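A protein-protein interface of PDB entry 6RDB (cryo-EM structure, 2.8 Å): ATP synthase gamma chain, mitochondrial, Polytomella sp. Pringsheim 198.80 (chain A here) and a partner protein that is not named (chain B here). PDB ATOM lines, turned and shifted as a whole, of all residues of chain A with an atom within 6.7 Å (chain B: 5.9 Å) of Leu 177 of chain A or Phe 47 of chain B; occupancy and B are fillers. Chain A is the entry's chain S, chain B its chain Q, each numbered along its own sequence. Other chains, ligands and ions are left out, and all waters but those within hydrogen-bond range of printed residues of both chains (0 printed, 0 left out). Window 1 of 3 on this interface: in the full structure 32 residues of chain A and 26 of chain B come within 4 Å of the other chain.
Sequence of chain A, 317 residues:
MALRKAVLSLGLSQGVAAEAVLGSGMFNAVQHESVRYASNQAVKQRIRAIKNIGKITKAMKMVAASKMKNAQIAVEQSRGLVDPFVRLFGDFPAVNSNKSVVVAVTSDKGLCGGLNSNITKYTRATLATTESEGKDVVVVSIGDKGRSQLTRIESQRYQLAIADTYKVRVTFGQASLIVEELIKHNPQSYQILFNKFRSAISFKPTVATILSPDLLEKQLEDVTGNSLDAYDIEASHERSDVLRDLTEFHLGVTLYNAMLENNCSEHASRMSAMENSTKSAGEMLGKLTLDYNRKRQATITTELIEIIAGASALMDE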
ATOM      1  N   ILE A 162       6.324 -31.392   3.642  1.00  0.00           N
ATOM      2  CA  ILE A 162       5.021 -30.839   3.296  1.00  0.00           C
ATOM      3  C   ILE A 162       4.089 -31.075   4.473  1.00  0.00           C
ATOM      4  O   ILE A 162       4.042 -32.180   5.022  1.00  0.00           O
ATOM      5  CB  ILE A 162       4.460 -31.472   2.008  1.00  0.00           C
ATOM      6  CG1 ILE A 162       5.347 -31.153   0.808  1.00  0.00           C
ATOM      7  CG2 ILE A 162       3.063 -30.976   1.713  1.00  0.00           C
ATOM      8  CD1 ILE A 162       6.185 -32.299   0.357  1.00  0.00           C
ATOM      9  N   ALA A 163       3.366 -30.040   4.884  1.00  0.00           N
ATOM     10  CA  ALA A 163       2.410 -30.169   5.966  1.00  0.00           C
ATOM     11  C   ALA A 163       1.213 -29.285   5.662  1.00  0.00           C
ATOM     12  O   ALA A 163       1.157 -28.629   4.618  1.00  0.00           O
ATOM     13  CB  ALA A 163       3.050 -29.816   7.310  1.00  0.00           C
ATOM     14  N   ASP A 164       0.250 -29.293   6.592  1.00  0.00           N
ATOM     15  CA  ASP A 164      -1.000 -28.528   6.521  1.00  0.00           C
ATOM     16  C   ASP A 164      -1.808 -28.859   5.271  1.00  0.00           C
ATOM     17  O   ASP A 164      -2.491 -27.997   4.715  1.00  0.00           O
ATOM     18  CB  ASP A 164      -0.745 -27.021   6.619  1.00  0.00           C
ATOM     19  CG  ASP A 164      -0.909 -26.493   8.029  1.00  0.00           C
ATOM     20  OD1 ASP A 164      -1.293 -27.281   8.921  1.00  0.00           O
ATOM     21  OD2 ASP A 164      -0.641 -25.292   8.247  1.00  0.00           O
ATOM     22  N   THR A 165      -1.747 -30.113   4.829  1.00  0.00           N
ATOM     23  CA  THR A 165      -2.366 -30.502   3.570  1.00  0.00           C
ATOM     24  C   THR A 165      -3.804 -30.976   3.719  1.00  0.00           C
ATOM     25  O   THR A 165      -4.588 -30.839   2.775  1.00  0.00           O
ATOM     26  CB  THR A 165      -1.533 -31.590   2.890  1.00  0.00           C
ATOM     27  OG1 THR A 165      -2.266 -32.127   1.785  1.00  0.00           O
ATOM     28  CG2 THR A 165      -1.176 -32.695   3.856  1.00  0.00           C
ATOM     29  N   TYR A 166      -4.179 -31.525   4.872  1.00  0.00           N
ATOM     30  CA  TYR A 166      -5.543 -31.969   5.113  1.00  0.00           C
ATOM     31  C   TYR A 166      -6.379 -30.922   5.824  1.00  0.00           C
ATOM     32  O   TYR A 166      -7.427 -31.263   6.385  1.00  0.00           O
ATOM     33  CB  TYR A 166      -5.545 -33.249   5.937  1.00  0.00           C
ATOM     34  CG  TYR A 166      -4.505 -34.241   5.529  1.00  0.00           C
ATOM     35  CD1 TYR A 166      -4.638 -34.971   4.366  1.00  0.00           C
ATOM     36  CD2 TYR A 166      -3.388 -34.463   6.321  1.00  0.00           C
ATOM     37  CE1 TYR A 166      -3.690 -35.885   3.997  1.00  0.00           C
ATOM     38  CE2 TYR A 166      -2.431 -35.382   5.956  1.00  0.00           C
ATOM     39  CZ  TYR A 166      -2.594 -36.088   4.790  1.00  0.00           C
ATOM     40  OH  TYR A 166      -1.657 -37.005   4.409  1.00  0.00           O
ATOM     41  N   PHE A 172      -6.341 -32.400  -6.476  1.00  0.00           N
ATOM     42  CA  PHE A 172      -5.311 -32.815  -7.421  1.00  0.00           C
ATOM     43  C   PHE A 172      -4.381 -31.669  -7.781  1.00  0.00           C
ATOM     44  O   PHE A 172      -3.197 -31.903  -8.041  1.00  0.00           O
ATOM     45  CB  PHE A 172      -5.942 -33.387  -8.685  1.00  0.00           C
ATOM     46  CG  PHE A 172      -4.992 -34.194  -9.513  1.00  0.00           C
ATOM     47  CD1 PHE A 172      -4.271 -33.613 -10.540  1.00  0.00           C
ATOM     48  CD2 PHE A 172      -4.812 -35.534  -9.255  1.00  0.00           C
ATOM     49  CE1 PHE A 172      -3.396 -34.354 -11.287  1.00  0.00           C
ATOM     50  CE2 PHE A 172      -3.944 -36.275 -10.001  1.00  0.00           C
ATOM     51  CZ  PHE A 172      -3.233 -35.687 -11.019  1.00  0.00           C
ATOM     52  N   GLY A 173      -4.893 -30.437  -7.822  1.00  0.00           N
ATOM     53  CA  GLY A 173      -4.028 -29.299  -8.071  1.00  0.00           C
ATOM     54  C   GLY A 173      -3.051 -29.054  -6.942  1.00  0.00           C
ATOM     55  O   GLY A 173      -1.927 -28.602  -7.175  1.00  0.00           O
ATOM     56  N   GLN A 174      -3.460 -29.360  -5.713  1.00  0.00           N
ATOM     57  CA  GLN A 174      -2.537 -29.317  -4.588  1.00  0.00           C
ATOM     58  C   GLN A 174      -1.531 -30.456  -4.666  1.00  0.00           C
ATOM     59  O   GLN A 174      -0.334 -30.250  -4.450  1.00  0.00           O
ATOM     60  CB  GLN A 174      -3.326 -29.366  -3.285  1.00  0.00           C
ATOM     61  CG  GLN A 174      -2.592 -29.937  -2.105  1.00  0.00           C
ATOM     62  CD  GLN A 174      -3.504 -30.118  -0.928  1.00  0.00           C
ATOM     63  OE1 GLN A 174      -4.697 -30.349  -1.085  1.00  0.00           O
ATOM     64  NE2 GLN A 174      -2.954 -30.001   0.262  1.00  0.00           N
ATOM     65  N   ALA A 175      -1.995 -31.656  -5.017  1.00  0.00           N
ATOM     66  CA  ALA A 175      -1.098 -32.793  -5.160  1.00  0.00           C
ATOM     67  C   ALA A 175      -0.224 -32.697  -6.399  1.00  0.00           C
ATOM     68  O   ALA A 175       0.751 -33.443  -6.510  1.00  0.00           O
ATOM     69  CB  ALA A 175      -1.897 -34.086  -5.200  1.00  0.00           C
ATOM     70  N   SER A 176      -0.556 -31.811  -7.340  1.00  0.00           N
ATOM     71  CA  SER A 176       0.338 -31.540  -8.457  1.00  0.00           C
ATOM     72  C   SER A 176       1.488 -30.639  -8.036  1.00  0.00           C
ATOM     73  O   SER A 176       2.636 -30.884  -8.418  1.00  0.00           O
ATOM     74  CB  SER A 176      -0.437 -30.909  -9.607  1.00  0.00           C
ATOM     75  OG  SER A 176      -1.494 -31.747 -10.028  1.00  0.00           O
ATOM     76  N   LEU A 177       1.197 -29.596  -7.248  1.00  0.00           N
ATOM     77  CA  LEU A 177       2.243 -28.715  -6.735  1.00  0.00           C
ATOM     78  C   LEU A 177       3.188 -29.445  -5.797  1.00  0.00           C
ATOM     79  O   LEU A 177       4.385 -29.149  -5.781  1.00  0.00           O
ATOM     80  CB  LEU A 177       1.628 -27.528  -6.002  1.00  0.00           C
ATOM     81  CG  LEU A 177       0.883 -26.493  -6.829  1.00  0.00           C
ATOM     82  CD1 LEU A 177       0.452 -25.351  -5.939  1.00  0.00           C
ATOM     83  CD2 LEU A 177       1.765 -25.998  -7.957  1.00  0.00           C
ATOM     84  N   ILE A 178       2.670 -30.384  -5.005  1.00  0.00           N
ATOM     85  CA  ILE A 178       3.531 -31.219  -4.177  1.00  0.00           C
ATOM     86  C   ILE A 178       4.369 -32.133  -5.055  1.00  0.00           C
ATOM     87  O   ILE A 178       5.546 -32.384  -4.772  1.00  0.00           O
ATOM     88  CB  ILE A 178       2.677 -32.004  -3.164  1.00  0.00           C
ATOM     89  CG1 ILE A 178       1.932 -31.038  -2.252  1.00  0.00           C
ATOM     90  CG2 ILE A 178       3.524 -32.889  -2.301  1.00  0.00           C
ATOM     91  CD1 ILE A 178       0.766 -31.651  -1.538  1.00  0.00           C
ATOM     92  N   VAL A 179       3.792 -32.608  -6.159  1.00  0.00           N
ATOM     93  CA  VAL A 179       4.556 -33.426  -7.090  1.00  0.00           C
ATOM     94  C   VAL A 179       5.564 -32.596  -7.866  1.00  0.00           C
ATOM     95  O   VAL A 179       6.693 -33.044  -8.061  1.00  0.00           O
ATOM     96  CB  VAL A 179       3.622 -34.157  -8.053  1.00  0.00           C
ATOM     97  N   GLU A 180       5.197 -31.370  -8.263  1.00  0.00           N
ATOM     98  CA  GLU A 180       6.090 -30.527  -9.059  1.00  0.00           C
ATOM     99  C   GLU A 180       7.330 -30.096  -8.286  1.00  0.00           C
ATOM    100  O   GLU A 180       8.364 -29.803  -8.894  1.00  0.00           O
ATOM    101  CB  GLU A 180       5.342 -29.300  -9.563  1.00  0.00           C
ATOM    102  CG  GLU A 180       4.488 -29.575 -10.773  1.00  0.00           C
ATOM    103  CD  GLU A 180       3.621 -28.400 -11.140  1.00  0.00           C
ATOM    104  OE1 GLU A 180       4.156 -27.277 -11.211  1.00  0.00           O
ATOM    105  OE2 GLU A 180       2.407 -28.601 -11.346  1.00  0.00           O
ATOM    106  N   GLU A 181       7.256 -30.062  -6.956  1.00  0.00           N
ATOM    107  CA  GLU A 181       8.442 -29.867  -6.138  1.00  0.00           C
ATOM    108  C   GLU A 181       9.335 -31.101  -6.093  1.00  0.00           C
ATOM    109  O   GLU A 181      10.468 -31.003  -5.615  1.00  0.00           O
ATOM    110  CB  GLU A 181       8.039 -29.473  -4.718  1.00  0.00           C
ATOM    111  CG  GLU A 181       7.268 -28.160  -4.621  1.00  0.00           C
ATOM    112  CD  GLU A 181       8.097 -26.938  -4.966  1.00  0.00           C
ATOM    113  OE1 GLU A 181       9.316 -26.940  -4.694  1.00  0.00           O
ATOM    114  OE2 GLU A 181       7.525 -25.968  -5.504  1.00  0.00           O
ATOM    115  N   LEU A 182       8.856 -32.254  -6.563  1.00  0.00           N
ATOM    116  CA  LEU A 182       9.670 -33.459  -6.656  1.00  0.00           C
ATOM    117  C   LEU A 182      10.235 -33.696  -8.051  1.00  0.00           C
ATOM    118  O   LEU A 182      10.947 -34.683  -8.246  1.00  0.00           O
ATOM    119  CB  LEU A 182       8.863 -34.689  -6.229  1.00  0.00           C
ATOM    120  CG  LEU A 182       8.172 -34.658  -4.865  1.00  0.00           C
ATOM    121  CD1 LEU A 182       7.573 -36.015  -4.565  1.00  0.00           C
ATOM    122  CD2 LEU A 182       9.132 -34.245  -3.771  1.00  0.00           C
ATOM    123  N   LEU A 255       0.341 -39.649  -5.926  1.00  0.00           N
ATOM    124  CA  LEU A 255       0.476 -38.778  -4.766  1.00  0.00           C
ATOM    125  C   LEU A 255      -0.881 -38.330  -4.256  1.00  0.00           C
ATOM    126  O   LEU A 255      -1.102 -38.267  -3.043  1.00  0.00           O
ATOM    127  CB  LEU A 255       1.326 -37.565  -5.113  1.00  0.00           C
ATOM    128  CG  LEU A 255       2.173 -36.987  -3.995  1.00  0.00           C
ATOM    129  CD1 LEU A 255       3.068 -38.058  -3.421  1.00  0.00           C
ATOM    130  CD2 LEU A 255       2.992 -35.851  -4.545  1.00  0.00           C
ATOM    131  N   ARG B  18       1.300 -28.764 -14.169  1.00  0.00           N
ATOM    132  CA  ARG B  18       0.764 -27.413 -14.072  1.00  0.00           C
ATOM    133  C   ARG B  18      -0.014 -27.043 -15.321  1.00  0.00           C
ATOM    134  O   ARG B  18      -0.991 -26.295 -15.239  1.00  0.00           O
ATOM    135  CB  ARG B  18       1.885 -26.404 -13.833  1.00  0.00           C
ATOM    136  CG  ARG B  18       1.387 -25.042 -13.382  1.00  0.00           C
ATOM    137  CD  ARG B  18       2.528 -24.081 -13.179  1.00  0.00           C
ATOM    138  NE  ARG B  18       3.455 -24.561 -12.167  1.00  0.00           N
ATOM    139  CZ  ARG B  18       3.353 -24.294 -10.872  1.00  0.00           C
ATOM    140  NH1 ARG B  18       2.357 -23.545 -10.420  1.00  0.00           N
ATOM    141  NH2 ARG B  18       4.251 -24.786 -10.031  1.00  0.00           N
ATOM    142  N   ILE B  45      -6.179 -24.891  -3.247  1.00  0.00           N
ATOM    143  CA  ILE B  45      -4.870 -25.428  -2.900  1.00  0.00           C
ATOM    144  C   ILE B  45      -4.471 -24.842  -1.555  1.00  0.00           C
ATOM    145  O   ILE B  45      -4.168 -23.646  -1.460  1.00  0.00           O
ATOM    146  CB  ILE B  45      -3.814 -25.116  -3.965  1.00  0.00           C
ATOM    147  CG1 ILE B  45      -4.196 -25.765  -5.293  1.00  0.00           C
ATOM    148  CG2 ILE B  45      -2.455 -25.604  -3.516  1.00  0.00           C
ATOM    149  CD1 ILE B  45      -3.282 -25.404  -6.428  1.00  0.00           C
ATOM    150  N   HIS B  46      -4.470 -25.675  -0.515  1.00  0.00           N
ATOM    151  CA  HIS B  46      -4.104 -25.245   0.834  1.00  0.00           C
ATOM    152  C   HIS B  46      -3.116 -26.255   1.400  1.00  0.00           C
ATOM    153  O   HIS B  46      -3.523 -27.320   1.873  1.00  0.00           O
ATOM    154  CB  HIS B  46      -5.326 -25.127   1.736  1.00  0.00           C
ATOM    155  CG  HIS B  46      -6.284 -24.055   1.329  1.00  0.00           C
ATOM    156  ND1 HIS B  46      -7.509 -24.330   0.761  1.00  0.00           N
ATOM    157  CD2 HIS B  46      -6.204 -22.708   1.418  1.00  0.00           C
ATOM    158  CE1 HIS B  46      -8.140 -23.198   0.514  1.00  0.00           C
ATOM    159  NE2 HIS B  46      -7.370 -22.199   0.904  1.00  0.00           N
ATOM    160  N   PHE B  47      -1.833 -25.920   1.361  1.00  0.00           N
ATOM    161  CA  PHE B  47      -0.811 -26.706   2.038  1.00  0.00           C
ATOM    162  C   PHE B  47       0.356 -25.779   2.346  1.00  0.00           C
ATOM    163  O   PHE B  47       0.255 -24.558   2.194  1.00  0.00           O
ATOM    164  CB  PHE B  47      -0.406 -27.936   1.210  1.00  0.00           C
ATOM    165  CG  PHE B  47       0.457 -27.635   0.016  1.00  0.00           C
ATOM    166  CD1 PHE B  47      -0.080 -27.063  -1.126  1.00  0.00           C
ATOM    167  CD2 PHE B  47       1.801 -27.967   0.021  1.00  0.00           C
ATOM    168  CE1 PHE B  47       0.713 -26.802  -2.219  1.00  0.00           C
ATOM    169  CE2 PHE B  47       2.598 -27.704  -1.068  1.00  0.00           C
ATOM    170  CZ  PHE B  47       2.052 -27.125  -2.190  1.00  0.00           C
ATOM    171  N   ARG B  48       1.457 -26.353   2.818  1.00  0.00           N
ATOM    172  CA  ARG B  48       2.677 -25.600   3.052  1.00  0.00           C
ATOM    173  C   ARG B  48       3.853 -26.548   2.894  1.00  0.00           C
ATOM    174  O   ARG B  48       3.702 -27.768   2.977  1.00  0.00           O
ATOM    175  CB  ARG B  48       2.679 -24.936   4.435  1.00  0.00           C
ATOM    176  CG  ARG B  48       2.782 -25.895   5.606  1.00  0.00           C
ATOM    177  CD  ARG B  48       2.954 -25.151   6.918  1.00  0.00           C
ATOM    178  NE  ARG B  48       3.957 -25.792   7.761  1.00  0.00           N
ATOM    179  CZ  ARG B  48       3.677 -26.620   8.761  1.00  0.00           C
ATOM    180  NH1 ARG B  48       4.660 -27.163   9.464  1.00  0.00           N
ATOM    181  NH2 ARG B  48       2.418 -26.909   9.059  1.00  0.00           N
ATOM    182  N   GLN B  49       5.031 -25.979   2.649  1.00  0.00           N
ATOM    183  CA  GLN B  49       6.225 -26.785   2.445  1.00  0.00           C
ATOM    184  C   GLN B  49       7.412 -26.112   3.112  1.00  0.00           C
ATOM    185  O   GLN B  49       7.378 -24.925   3.443  1.00  0.00           O
ATOM    186  CB  GLN B  49       6.511 -27.017   0.955  1.00  0.00           C
ATOM    187  CG  GLN B  49       7.216 -25.871   0.271  1.00  0.00           C
ATOM    188  CD  GLN B  49       7.279 -26.032  -1.229  1.00  0.00           C
ATOM    189  OE1 GLN B  49       6.434 -25.513  -1.957  1.00  0.00           O
ATOM    190  NE2 GLN B  49       8.287 -26.754  -1.704  1.00  0.00           N
ATOM    191  N   LYS B  61       7.292 -21.914   3.197  1.00  0.00           N
ATOM    192  CA  LYS B  61       6.499 -21.542   2.037  1.00  0.00           C
ATOM    193  C   LYS B  61       5.062 -21.946   2.311  1.00  0.00           C
ATOM    194  O   LYS B  61       4.809 -23.077   2.728  1.00  0.00           O
ATOM    195  CB  LYS B  61       7.013 -22.229   0.767  1.00  0.00           C
ATOM    196  CG  LYS B  61       6.251 -21.861  -0.486  1.00  0.00           C
ATOM    197  CD  LYS B  61       6.643 -20.480  -0.976  1.00  0.00           C
ATOM    198  CE  LYS B  61       5.788 -20.048  -2.149  1.00  0.00           C
ATOM    199  NZ  LYS B  61       5.861 -21.028  -3.261  1.00  0.00           N
ATOM    200  N   VAL B  62       4.126 -21.026   2.077  1.00  0.00           N
ATOM    201  CA  VAL B  62       2.727 -21.233   2.423  1.00  0.00           C
ATOM    202  C   VAL B  62       1.870 -20.983   1.190  1.00  0.00           C
ATOM    203  O   VAL B  62       1.996 -19.964   0.510  1.00  0.00           O
ATOM    204  CB  VAL B  62       2.284 -20.317   3.594  1.00  0.00           C
ATOM    205  CG1 VAL B  62       0.769 -20.322   3.777  1.00  0.00           C
ATOM    206  CG2 VAL B  62       2.970 -20.736   4.890  1.00  0.00           C
ATOM    207  N   TYR B  63       0.993 -21.944   0.903  1.00  0.00           N
ATOM    208  CA  TYR B  63       0.018 -21.827  -0.169  1.00  0.00           C
ATOM    209  C   TYR B  63      -1.355 -21.690   0.464  1.00  0.00           C
ATOM    210  O   TYR B  63      -1.722 -22.494   1.326  1.00  0.00           O
ATOM    211  CB  TYR B  63       0.050 -23.048  -1.092  1.00  0.00           C
ATOM    212  CG  TYR B  63       1.311 -23.190  -1.913  1.00  0.00           C
ATOM    213  CD1 TYR B  63       2.469 -23.728  -1.363  1.00  0.00           C
ATOM    214  CD2 TYR B  63       1.340 -22.800  -3.242  1.00  0.00           C
ATOM    215  CE1 TYR B  63       3.619 -23.863  -2.111  1.00  0.00           C
ATOM    216  CE2 TYR B  63       2.485 -22.933  -4.000  1.00  0.00           C
ATOM    217  CZ  TYR B  63       3.622 -23.465  -3.428  1.00  0.00           C
ATOM    218  OH  TYR B  63       4.764 -23.595  -4.180  1.00  0.00           O
ATOM    219  N   GLU B  64      -2.104 -20.670   0.056  1.00  0.00           N
ATOM    220  CA  GLU B  64      -3.442 -20.466   0.594  1.00  0.00           C
ATOM    221  C   GLU B  64      -4.398 -20.064  -0.526  1.00  0.00           C
ATOM    222  O   GLU B  64      -5.235 -19.178  -0.358  1.00  0.00           O
ATOM    223  CB  GLU B  64      -3.407 -19.433   1.726  1.00  0.00           C
ATOM    224  CG  GLU B  64      -4.436 -19.643   2.850  1.00  0.00           C
ATOM    225  CD  GLU B  64      -5.739 -18.887   2.674  1.00  0.00           C
ATOM    226  OE1 GLU B  64      -5.727 -17.788   2.090  1.00  0.00           O
ATOM    227  OE2 GLU B  64      -6.782 -19.391   3.140  1.00  0.00           O
ATOM    228  N   LEU B  65      -4.262 -20.699  -1.691  1.00  0.00           N
ATOM    229  CA  LEU B  65      -5.055 -20.346  -2.860  1.00  0.00           C
ATOM    230  C   LEU B  65      -6.417 -21.020  -2.804  1.00  0.00           C
ATOM    231  O   LEU B  65      -6.559 -22.120  -2.267  1.00  0.00           O
ATOM    232  CB  LEU B  65      -4.342 -20.752  -4.151  1.00  0.00           C
ATOM    233  CG  LEU B  65      -2.934 -20.226  -4.443  1.00  0.00           C
ATOM    234  CD1 LEU B  65      -1.845 -21.173  -3.946  1.00  0.00           C
ATOM    235  CD2 LEU B  65      -2.762 -19.926  -5.925  1.00  0.00           C
ATOM    236  N   ILE B  69      -4.493 -23.420  -9.531  1.00  0.00           N
ATOM    237  CA  ILE B  69      -3.040 -23.444  -9.658  1.00  0.00           C
ATOM    238  C   ILE B  69      -2.626 -22.090 -10.232  1.00  0.00           C
ATOM    239  O   ILE B  69      -3.421 -21.458 -10.948  1.00  0.00           O
ATOM    240  CB  ILE B  69      -2.590 -24.658 -10.502  1.00  0.00           C
ATOM    241  CG1 ILE B  69      -1.303 -25.276  -9.957  1.00  0.00           C
ATOM    242  CG2 ILE B  69      -2.399 -24.320 -11.976  1.00  0.00           C
ATOM    243  CD1 ILE B  69      -1.032 -26.667 -10.472  1.00  0.00           C
ATOM    244  N   PRO B  70      -1.456 -21.556  -9.874  1.00  0.00           N
ATOM    245  CA  PRO B  70      -1.062 -20.234 -10.385  1.00  0.00           C
ATOM    246  C   PRO B  70      -0.753 -20.264 -11.876  1.00  0.00           C
ATOM    247  O   PRO B  70      -0.012 -21.124 -12.357  1.00  0.00           O
ATOM    248  CB  PRO B  70       0.181 -19.890  -9.559  1.00  0.00           C
ATOM    249  CG  PRO B  70       0.029 -20.677  -8.316  1.00  0.00           C
ATOM    250  CD  PRO B  70      -0.631 -21.953  -8.719  1.00  0.00           C
ATOM    251  N   ASN B  74       6.136 -20.085 -11.403  1.00  0.00           N
ATOM    252  CA  ASN B  74       6.404 -20.455 -10.019  1.00  0.00           C
ATOM    253  C   ASN B  74       7.860 -20.190  -9.657  1.00  0.00           C
ATOM    254  O   ASN B  74       8.160 -19.664  -8.586  1.00  0.00           O
ATOM    255  CB  ASN B  74       6.070 -21.929  -9.787  1.00  0.00           C
ATOM    256  CG  ASN B  74       5.973 -22.283  -8.314  1.00  0.00           C
ATOM    257  OD1 ASN B  74       5.180 -21.700  -7.575  1.00  0.00           O
ATOM    258  ND2 ASN B  74       6.779 -23.244  -7.883  1.00  0.00           N
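OE1 of Glu 180 of chain A is in salt-bridge range of NH2 of Arg 18 of chain B (2.8 Å). The backbone carbonyl oxygen (O) of His 46 of chain B sits at hydrogen-bond distance from the side-chain amide nitrogen (NE2) of Gln 174 of chain A (3.2 Å). O of Ala 163 of chain A lies within hydrogen-bond range of N of Arg 48 of chain B (2.9 Å). The guanidinium group (NH2) of Arg 48 of chain B is in salt-bridge range of the side-chain carboxylate (OD2) of Asp 164 of chain A, 3.6 Å away. The side-chain carboxylate of Glu 181 of chain A lies within hydrogen-bond range of the side-chain amide nitrogen of Gln 49 of chain B, at 3.2 Å. O of Asp 164 of chain A sits close to O of His 46 of chain B (3.1 Å).
The backbone carbonyl oxygen (O) of Ile 45 of chain B sits at hydrogen-bond distance from the backbone NH (N) of Leu 65 of chain B. O of Leu 65 of chain B sits at hydrogen-bond distance from NE2 of His 46 of chain B, at 3.3 Å. The backbone NH (N) of Gln 49 of chain B lies within hydrogen-bond range of the backbone carbonyl oxygen (O) of Lys 61 of chain B (2.9 Å). The side-chain amide oxygen of Gln 49 of chain B sits close to the side-chain hydroxyl of Tyr 63 of chain B (3.4 Å). OH of Tyr 63 of chain B lies within hydrogen-bond range of NZ of Lys 61 of chain B (2.9 Å). OG1 of Thr 165 of chain A sits at hydrogen-bond distance from NE2 of Gln 174 of chain A, at 2.7 Å.
CG2 of Ile 162 of chain A touches CD2 of Phe 47 of chain B (3.7 Å). Phe 47 of chain B touches Ala 163 of chain A. O of Thr 165 of chain A touches O of His 46 of chain B (3.8 Å). Gly 173 of chain A touches Ile 45 of chain B (O to CD1, 3.6 Å). Gly 173 of chain A touches Ile 69 of chain B (O to CD1, 3.9 Å). CG1 of Ile 45 of chain B touches N of Gln 174 of chain A (3.7 Å). Gln 174 of chain A touches Phe 47 of chain B (NE2 to CB, 3.4 Å). Leu 177 of chain A touches Arg 18 of chain B. CD1 of Leu 177 of chain A touches CE2 of Tyr 63 of chain B, at 3.7 Å. CG1 of Ile 178 of chain A touches CE2 of Phe 47 of chain B, at 3.6 Å.
Printed residues of chain A within 4 Å of Phe 47 of chain B: Ile 162, Ala 163, Asp 164, Thr 165, Gln 174, Leu 177 and Ile 178. Of the printed residues of chain A, Ile 69 of chain B touches Gly 173 and Leu 177. Of the printed residues of chain A, His 46 of chain B touches Asp 164, Thr 165 and Gln 174. Printed residues of chain B within 4 Å of Gln 174 of chain A: Ile 45 (3.7 Å), His 46 (3.2 Å) and Phe 47 (3.4 Å). Printed residues of chain A within 4 Å of Tyr 63 of chain B: Leu 177 and Glu 181. Leu 182 of chain A touches none of the printed residues of chain B. Leu 65 of chain B touches none of the printed residues of chain A. The nearest residue of chain B that does not touch Leu 177 of chain A is Pro 70 of chain B (4.5 Å). The nearest printed residue of chain A that does not touch Phe 47 of chain B is Glu 181 of chain A (5.8 Å).
Of the 14 printed residues of chain B, 9 touch a printed residue of chain A. Of the 17 printed residues of chain A, 10 touch a printed residue of chain B. Printed residues of chain A that touch a printed residue of chain B: Ile 162, Ala 163, Asp 164, Thr 165, Gly 173, Gln 174, Leu 177, Ile 178, Glu 180 and Glu 181. Along chain A the printed residues that touch a printed residue of chain B span positions 162 to 181. Among the printed residues, Asp or Glu carboxylates within 4 Å of a Lys or Arg side-chain nitrogen of the other chain: Asp 164 of chain A with Arg 48 of chain B (3.6 Å) and Glu 180 of chain A with Arg 18 of chain B (2.8 Å).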
